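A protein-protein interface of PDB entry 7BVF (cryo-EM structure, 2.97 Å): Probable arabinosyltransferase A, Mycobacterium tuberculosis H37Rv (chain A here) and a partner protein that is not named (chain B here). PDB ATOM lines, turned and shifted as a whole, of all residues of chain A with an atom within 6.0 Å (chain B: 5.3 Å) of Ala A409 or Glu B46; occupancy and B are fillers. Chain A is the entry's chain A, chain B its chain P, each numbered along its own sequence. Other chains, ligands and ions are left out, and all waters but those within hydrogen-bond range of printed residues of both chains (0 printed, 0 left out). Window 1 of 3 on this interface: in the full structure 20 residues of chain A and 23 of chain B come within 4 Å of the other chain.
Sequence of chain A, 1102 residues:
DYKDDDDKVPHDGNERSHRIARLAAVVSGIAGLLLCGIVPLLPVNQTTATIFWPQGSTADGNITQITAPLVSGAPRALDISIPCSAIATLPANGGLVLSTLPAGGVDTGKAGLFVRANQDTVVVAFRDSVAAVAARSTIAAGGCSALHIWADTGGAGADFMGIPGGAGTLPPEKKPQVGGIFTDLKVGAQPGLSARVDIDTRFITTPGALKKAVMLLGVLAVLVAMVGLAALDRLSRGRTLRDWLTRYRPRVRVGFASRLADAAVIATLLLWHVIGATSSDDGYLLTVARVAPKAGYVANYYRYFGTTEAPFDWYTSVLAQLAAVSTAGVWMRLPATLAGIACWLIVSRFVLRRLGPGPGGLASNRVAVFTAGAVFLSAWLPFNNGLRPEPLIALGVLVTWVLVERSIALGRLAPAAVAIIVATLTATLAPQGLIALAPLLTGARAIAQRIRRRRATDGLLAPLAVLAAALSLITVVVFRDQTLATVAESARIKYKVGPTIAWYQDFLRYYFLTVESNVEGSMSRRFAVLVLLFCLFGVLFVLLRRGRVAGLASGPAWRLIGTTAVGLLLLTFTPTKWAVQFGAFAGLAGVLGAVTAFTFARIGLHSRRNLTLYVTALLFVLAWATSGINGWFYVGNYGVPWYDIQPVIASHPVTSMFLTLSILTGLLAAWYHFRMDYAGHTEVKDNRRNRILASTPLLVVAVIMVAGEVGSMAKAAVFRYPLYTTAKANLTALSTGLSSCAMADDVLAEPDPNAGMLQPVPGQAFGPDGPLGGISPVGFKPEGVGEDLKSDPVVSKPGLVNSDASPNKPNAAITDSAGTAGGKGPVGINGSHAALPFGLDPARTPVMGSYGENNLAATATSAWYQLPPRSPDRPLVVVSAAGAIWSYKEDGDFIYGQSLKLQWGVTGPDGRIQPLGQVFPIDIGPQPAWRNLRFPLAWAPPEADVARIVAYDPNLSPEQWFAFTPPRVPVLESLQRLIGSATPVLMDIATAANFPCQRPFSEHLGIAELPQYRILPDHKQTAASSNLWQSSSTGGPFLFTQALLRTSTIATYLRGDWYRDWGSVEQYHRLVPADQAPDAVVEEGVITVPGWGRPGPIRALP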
ATOM      1  N   ARG A 354       3.563  -8.622 -22.874  1.00  0.00           N
ATOM      2  CA  ARG A 354       4.680  -8.846 -23.782  1.00  0.00           C
ATOM      3  C   ARG A 354       5.647  -7.670 -23.773  1.00  0.00           C
ATOM      4  O   ARG A 354       6.840  -7.846 -24.038  1.00  0.00           O
ATOM      5  CB  ARG A 354       4.155  -9.102 -25.193  1.00  0.00           C
ATOM      6  CG  ARG A 354       5.216  -9.437 -26.216  1.00  0.00           C
ATOM      7  CD  ARG A 354       5.676 -10.869 -26.087  1.00  0.00           C
ATOM      8  NE  ARG A 354       6.671 -11.201 -27.099  1.00  0.00           N
ATOM      9  CZ  ARG A 354       7.978 -11.260 -26.873  1.00  0.00           C
ATOM     10  NH1 ARG A 354       8.455 -11.012 -25.662  1.00  0.00           N
ATOM     11  NH2 ARG A 354       8.808 -11.568 -27.857  1.00  0.00           N
ATOM     12  N   VAL A 404       2.305 -13.544 -34.559  1.00  0.00           N
ATOM     13  CA  VAL A 404       3.681 -13.328 -34.993  1.00  0.00           C
ATOM     14  C   VAL A 404       4.613 -13.205 -33.793  1.00  0.00           C
ATOM     15  O   VAL A 404       5.727 -13.743 -33.800  1.00  0.00           O
ATOM     16  CB  VAL A 404       3.762 -12.093 -35.907  1.00  0.00           C
ATOM     17  CG1 VAL A 404       5.192 -11.638 -36.063  1.00  0.00           C
ATOM     18  CG2 VAL A 404       3.163 -12.407 -37.258  1.00  0.00           C
ATOM     19  N   GLU A 405       4.180 -12.508 -32.739  1.00  0.00           N
ATOM     20  CA  GLU A 405       5.021 -12.381 -31.553  1.00  0.00           C
ATOM     21  C   GLU A 405       5.204 -13.721 -30.858  1.00  0.00           C
ATOM     22  O   GLU A 405       6.294 -14.025 -30.367  1.00  0.00           O
ATOM     23  CB  GLU A 405       4.427 -11.362 -30.588  1.00  0.00           C
ATOM     24  CG  GLU A 405       4.607  -9.926 -31.025  1.00  0.00           C
ATOM     25  CD  GLU A 405       6.059  -9.502 -31.080  1.00  0.00           C
ATOM     26  OE1 GLU A 405       6.878 -10.051 -30.319  1.00  0.00           O
ATOM     27  OE2 GLU A 405       6.383  -8.613 -31.891  1.00  0.00           O
ATOM     28  N   ARG A 406       4.150 -14.532 -30.802  1.00  0.00           N
ATOM     29  CA  ARG A 406       4.269 -15.867 -30.228  1.00  0.00           C
ATOM     30  C   ARG A 406       5.239 -16.726 -31.030  1.00  0.00           C
ATOM     31  O   ARG A 406       6.029 -17.487 -30.459  1.00  0.00           O
ATOM     32  CB  ARG A 406       2.891 -16.516 -30.167  1.00  0.00           C
ATOM     33  CG  ARG A 406       2.834 -17.800 -29.392  1.00  0.00           C
ATOM     34  CD  ARG A 406       1.402 -18.259 -29.228  1.00  0.00           C
ATOM     35  NE  ARG A 406       1.315 -19.469 -28.422  1.00  0.00           N
ATOM     36  CZ  ARG A 406       1.252 -19.474 -27.097  1.00  0.00           C
ATOM     37  NH1 ARG A 406       1.177 -20.622 -26.440  1.00  0.00           N
ATOM     38  NH2 ARG A 406       1.263 -18.331 -26.428  1.00  0.00           N
ATOM     39  N   SER A 407       5.201 -16.609 -32.357  1.00  0.00           N
ATOM     40  CA  SER A 407       6.119 -17.370 -33.197  1.00  0.00           C
ATOM     41  C   SER A 407       7.559 -16.922 -32.996  1.00  0.00           C
ATOM     42  O   SER A 407       8.471 -17.754 -32.952  1.00  0.00           O
ATOM     43  CB  SER A 407       5.721 -17.230 -34.664  1.00  0.00           C
ATOM     44  OG  SER A 407       6.721 -17.750 -35.515  1.00  0.00           O
ATOM     45  N   ILE A 408       7.787 -15.615 -32.885  1.00  0.00           N
ATOM     46  CA  ILE A 408       9.144 -15.115 -32.686  1.00  0.00           C
ATOM     47  C   ILE A 408       9.672 -15.523 -31.315  1.00  0.00           C
ATOM     48  O   ILE A 408      10.835 -15.918 -31.178  1.00  0.00           O
ATOM     49  CB  ILE A 408       9.184 -13.588 -32.873  1.00  0.00           C
ATOM     50  CG1 ILE A 408       9.038 -13.230 -34.348  1.00  0.00           C
ATOM     51  CG2 ILE A 408      10.469 -13.025 -32.328  1.00  0.00           C
ATOM     52  CD1 ILE A 408       9.024 -11.754 -34.609  1.00  0.00           C
ATOM     53  N   ALA A 409       8.830 -15.447 -30.285  1.00  0.00           N
ATOM     54  CA  ALA A 409       9.270 -15.775 -28.934  1.00  0.00           C
ATOM     55  C   ALA A 409       9.541 -17.266 -28.784  1.00  0.00           C
ATOM     56  O   ALA A 409      10.661 -17.673 -28.463  1.00  0.00           O
ATOM     57  CB  ALA A 409       8.227 -15.314 -27.918  1.00  0.00           C
ATOM     58  N   LEU A 410       8.525 -18.100 -29.014  1.00  0.00           N
ATOM     59  CA  LEU A 410       8.669 -19.526 -28.739  1.00  0.00           C
ATOM     60  C   LEU A 410       9.699 -20.202 -29.631  1.00  0.00           C
ATOM     61  O   LEU A 410      10.174 -21.289 -29.291  1.00  0.00           O
ATOM     62  CB  LEU A 410       7.325 -20.232 -28.899  1.00  0.00           C
ATOM     63  CG  LEU A 410       6.216 -19.867 -27.919  1.00  0.00           C
ATOM     64  CD1 LEU A 410       4.942 -20.578 -28.309  1.00  0.00           C
ATOM     65  CD2 LEU A 410       6.615 -20.230 -26.507  1.00  0.00           C
ATOM     66  N   GLY A 411      10.053 -19.596 -30.756  1.00  0.00           N
ATOM     67  CA  GLY A 411      10.910 -20.264 -31.715  1.00  0.00           C
ATOM     68  C   GLY A 411      10.185 -21.295 -32.547  1.00  0.00           C
ATOM     69  O   GLY A 411      10.720 -22.382 -32.785  1.00  0.00           O
ATOM     70  N   ARG A 412       8.974 -20.983 -32.994  1.00  0.00           N
ATOM     71  CA  ARG A 412       8.140 -21.903 -33.748  1.00  0.00           C
ATOM     72  C   ARG A 412       7.704 -21.237 -35.042  1.00  0.00           C
ATOM     73  O   ARG A 412       7.849 -20.027 -35.224  1.00  0.00           O
ATOM     74  CB  ARG A 412       6.915 -22.337 -32.937  1.00  0.00           C
ATOM     75  CG  ARG A 412       7.231 -23.296 -31.814  1.00  0.00           C
ATOM     76  CD  ARG A 412       6.022 -23.528 -30.937  1.00  0.00           C
ATOM     77  NE  ARG A 412       6.293 -24.512 -29.898  1.00  0.00           N
ATOM     78  CZ  ARG A 412       5.446 -24.818 -28.922  1.00  0.00           C
ATOM     79  NH1 ARG A 412       4.270 -24.214 -28.848  1.00  0.00           N
ATOM     80  NH2 ARG A 412       5.774 -25.728 -28.018  1.00  0.00           N
ATOM     81  N   ARG A 559       8.728  -3.394 -33.039  1.00  0.00           N
ATOM     82  CA  ARG A 559       7.796  -4.020 -33.972  1.00  0.00           C
ATOM     83  C   ARG A 559       6.422  -3.365 -33.927  1.00  0.00           C
ATOM     84  O   ARG A 559       5.743  -3.292 -34.952  1.00  0.00           O
ATOM     85  CB  ARG A 559       7.695  -5.516 -33.691  1.00  0.00           C
ATOM     86  CG  ARG A 559       8.947  -6.272 -34.074  1.00  0.00           C
ATOM     87  CD  ARG A 559       8.800  -7.761 -33.879  1.00  0.00           C
ATOM     88  NE  ARG A 559      10.051  -8.353 -33.420  1.00  0.00           N
ATOM     89  CZ  ARG A 559      10.195  -9.003 -32.272  1.00  0.00           C
ATOM     90  NH1 ARG A 559       9.160  -9.165 -31.463  1.00  0.00           N
ATOM     91  NH2 ARG A 559      11.375  -9.503 -31.936  1.00  0.00           N
ATOM     92  N   VAL B  19      15.236  -9.321 -23.473  1.00  0.00           N
ATOM     93  CA  VAL B  19      13.953 -10.014 -23.564  1.00  0.00           C
ATOM     94  C   VAL B  19      12.897  -9.378 -22.668  1.00  0.00           C
ATOM     95  O   VAL B  19      11.769  -9.147 -23.105  1.00  0.00           O
ATOM     96  CB  VAL B  19      14.149 -11.506 -23.238  1.00  0.00           C
ATOM     97  CG1 VAL B  19      12.826 -12.159 -22.924  1.00  0.00           C
ATOM     98  CG2 VAL B  19      14.822 -12.208 -24.397  1.00  0.00           C
ATOM     99  N   SER B  41       6.247 -18.530 -18.541  1.00  0.00           N
ATOM    100  CA  SER B  41       6.683 -19.581 -19.453  1.00  0.00           C
ATOM    101  C   SER B  41       7.179 -19.003 -20.773  1.00  0.00           C
ATOM    102  O   SER B  41       8.185 -19.470 -21.320  1.00  0.00           O
ATOM    103  CB  SER B  41       5.540 -20.568 -19.688  1.00  0.00           C
ATOM    104  OG  SER B  41       5.926 -21.608 -20.568  1.00  0.00           O
ATOM    105  N   LEU B  42       6.498 -17.980 -21.293  1.00  0.00           N
ATOM    106  CA  LEU B  42       6.900 -17.401 -22.570  1.00  0.00           C
ATOM    107  C   LEU B  42       8.289 -16.785 -22.479  1.00  0.00           C
ATOM    108  O   LEU B  42       9.129 -16.995 -23.362  1.00  0.00           O
ATOM    109  CB  LEU B  42       5.879 -16.357 -23.020  1.00  0.00           C
ATOM    110  CG  LEU B  42       5.954 -15.907 -24.481  1.00  0.00           C
ATOM    111  CD1 LEU B  42       5.432 -16.992 -25.403  1.00  0.00           C
ATOM    112  CD2 LEU B  42       5.198 -14.609 -24.703  1.00  0.00           C
ATOM    113  N   SER B  43       8.561 -16.041 -21.406  1.00  0.00           N
ATOM    114  CA  SER B  43       9.870 -15.418 -21.260  1.00  0.00           C
ATOM    115  C   SER B  43      10.951 -16.455 -20.982  1.00  0.00           C
ATOM    116  O   SER B  43      12.079 -16.323 -21.469  1.00  0.00           O
ATOM    117  CB  SER B  43       9.834 -14.368 -20.155  1.00  0.00           C
ATOM    118  OG  SER B  43       9.359 -13.134 -20.651  1.00  0.00           O
ATOM    119  N   MET B  44      10.630 -17.494 -20.209  1.00  0.00           N
ATOM    120  CA  MET B  44      11.609 -18.550 -19.972  1.00  0.00           C
ATOM    121  C   MET B  44      12.010 -19.229 -21.276  1.00  0.00           C
ATOM    122  O   MET B  44      13.200 -19.441 -21.541  1.00  0.00           O
ATOM    123  CB  MET B  44      11.052 -19.571 -18.982  1.00  0.00           C
ATOM    124  CG  MET B  44      11.542 -19.394 -17.558  1.00  0.00           C
ATOM    125  SD  MET B  44      13.316 -19.095 -17.448  1.00  0.00           S
ATOM    126  CE  MET B  44      13.971 -20.614 -18.133  1.00  0.00           C
ATOM    127  N   VAL B  45      11.027 -19.568 -22.114  1.00  0.00           N
ATOM    128  CA  VAL B  45      11.355 -20.212 -23.381  1.00  0.00           C
ATOM    129  C   VAL B  45      12.071 -19.250 -24.317  1.00  0.00           C
ATOM    130  O   VAL B  45      12.954 -19.662 -25.073  1.00  0.00           O
ATOM    131  CB  VAL B  45      10.098 -20.806 -24.039  1.00  0.00           C
ATOM    132  CG1 VAL B  45      10.486 -21.628 -25.244  1.00  0.00           C
ATOM    133  CG2 VAL B  45       9.369 -21.688 -23.057  1.00  0.00           C
ATOM    134  N   GLU B  46      11.731 -17.959 -24.286  1.00  0.00           N
ATOM    135  CA  GLU B  46      12.445 -17.020 -25.145  1.00  0.00           C
ATOM    136  C   GLU B  46      13.903 -16.885 -24.725  1.00  0.00           C
ATOM    137  O   GLU B  46      14.791 -16.775 -25.576  1.00  0.00           O
ATOM    138  CB  GLU B  46      11.759 -15.658 -25.136  1.00  0.00           C
ATOM    139  CG  GLU B  46      12.191 -14.769 -26.283  1.00  0.00           C
ATOM    140  CD  GLU B  46      11.509 -13.420 -26.262  1.00  0.00           C
ATOM    141  OE1 GLU B  46      10.800 -13.131 -25.277  1.00  0.00           O
ATOM    142  OE2 GLU B  46      11.680 -12.648 -27.230  1.00  0.00           O
ATOM    143  N   ILE B  47      14.171 -16.906 -23.420  1.00  0.00           N
ATOM    144  CA  ILE B  47      15.551 -16.866 -22.948  1.00  0.00           C
ATOM    145  C   ILE B  47      16.292 -18.131 -23.367  1.00  0.00           C
ATOM    146  O   ILE B  47      17.428 -18.073 -23.853  1.00  0.00           O
ATOM    147  CB  ILE B  47      15.594 -16.666 -21.425  1.00  0.00           C
ATOM    148  CG1 ILE B  47      15.113 -15.264 -21.063  1.00  0.00           C
ATOM    149  CG2 ILE B  47      16.991 -16.894 -20.897  1.00  0.00           C
ATOM    150  CD1 ILE B  47      14.889 -15.070 -19.591  1.00  0.00           C
ATOM    151  N   ALA B  48      15.659 -19.292 -23.190  1.00  0.00           N
ATOM    152  CA  ALA B  48      16.309 -20.540 -23.575  1.00  0.00           C
ATOM    153  C   ALA B  48      16.512 -20.652 -25.078  1.00  0.00           C
ATOM    154  O   ALA B  48      17.395 -21.394 -25.517  1.00  0.00           O
ATOM    155  CB  ALA B  48      15.501 -21.734 -23.074  1.00  0.00           C
ATOM    156  N   VAL B  49      15.717 -19.942 -25.875  1.00  0.00           N
ATOM    157  CA  VAL B  49      15.891 -19.977 -27.323  1.00  0.00           C
ATOM    158  C   VAL B  49      16.972 -18.998 -27.763  1.00  0.00           C
ATOM    159  O   VAL B  49      17.780 -19.308 -28.642  1.00  0.00           O
ATOM    160  CB  VAL B  49      14.549 -19.698 -28.023  1.00  0.00           C
ATOM    161  CG1 VAL B  49      14.766 -19.346 -29.476  1.00  0.00           C
ATOM    162  CG2 VAL B  49      13.643 -20.906 -27.912  1.00  0.00           C
ATOM    163  N   GLN B  50      17.017 -17.812 -27.159  1.00  0.00           N
ATOM    164  CA  GLN B  50      18.023 -16.830 -27.535  1.00  0.00           C
ATOM    165  C   GLN B  50      19.394 -17.120 -26.944  1.00  0.00           C
ATOM    166  O   GLN B  50      20.379 -16.535 -27.404  1.00  0.00           O
ATOM    167  CB  GLN B  50      17.579 -15.431 -27.123  1.00  0.00           C
ATOM    168  CG  GLN B  50      16.642 -14.779 -28.110  1.00  0.00           C
ATOM    169  CD  GLN B  50      16.750 -13.274 -28.100  1.00  0.00           C
ATOM    170  OE1 GLN B  50      17.696 -12.713 -27.551  1.00  0.00           O
ATOM    171  NE2 GLN B  50      15.779 -12.608 -28.710  1.00  0.00           N
ATOM    172  N   THR B  51      19.488 -17.989 -25.939  1.00  0.00           N
ATOM    173  CA  THR B  51      20.798 -18.417 -25.469  1.00  0.00           C
ATOM    174  C   THR B  51      21.368 -19.565 -26.286  1.00  0.00           C
ATOM    175  O   THR B  51      22.523 -19.943 -26.070  1.00  0.00           O
ATOM    176  CB  THR B  51      20.735 -18.833 -24.002  1.00  0.00           C
ATOM    177  OG1 THR B  51      22.061 -18.877 -23.467  1.00  0.00           O
ATOM    178  CG2 THR B  51      20.116 -20.203 -23.873  1.00  0.00           C
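OE2 of Glu B46 lies within salt-bridge range of NH2 of Arg A354.
NE of Arg A354 lies within salt-bridge range of OE1 of Glu A405.
Ala A409 touches Glu B46 (O to CA, 3.8 Å). CD1 of Leu B42 touches CD2 of Leu A410, 3.6 Å away. Leu A410 touches Val B49 (O to CG2, 3.8 Å).
Printed residues of chain B within 4 Å of Arg A354: Glu B46 (3.1 Å). Ala A409 touches just one residue of chain B: Glu B46. Printed residues of chain B within 4 Å of Leu A410: Leu B42 (3.6 Å) and Val B49 (3.8 Å). Printed residues of chain A within 4 Å of Leu B42: Leu A410. Glu B46 touches just these residues of chain A: Arg A354 (3.1 Å) and Ala A409 (3.8 Å). Of the printed residues of chain A, Val B49 touches Leu A410 (3.8 Å). The nearest residue of chain A that does not touch Glu B46 is Ile A408 (5.2 Å). The nearest printed residue of chain B that does not touch Arg A354 is Leu B42 (4.02 Å).
Hydrophobic or aromatic side chains of chain B that line the printed part of chain A: Leu B42 and Val B49. Hydrophobic or aromatic side chains of chain A that line the printed part of chain B: Leu A410. Among the printed residues, 4 pairs touch across the chains.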
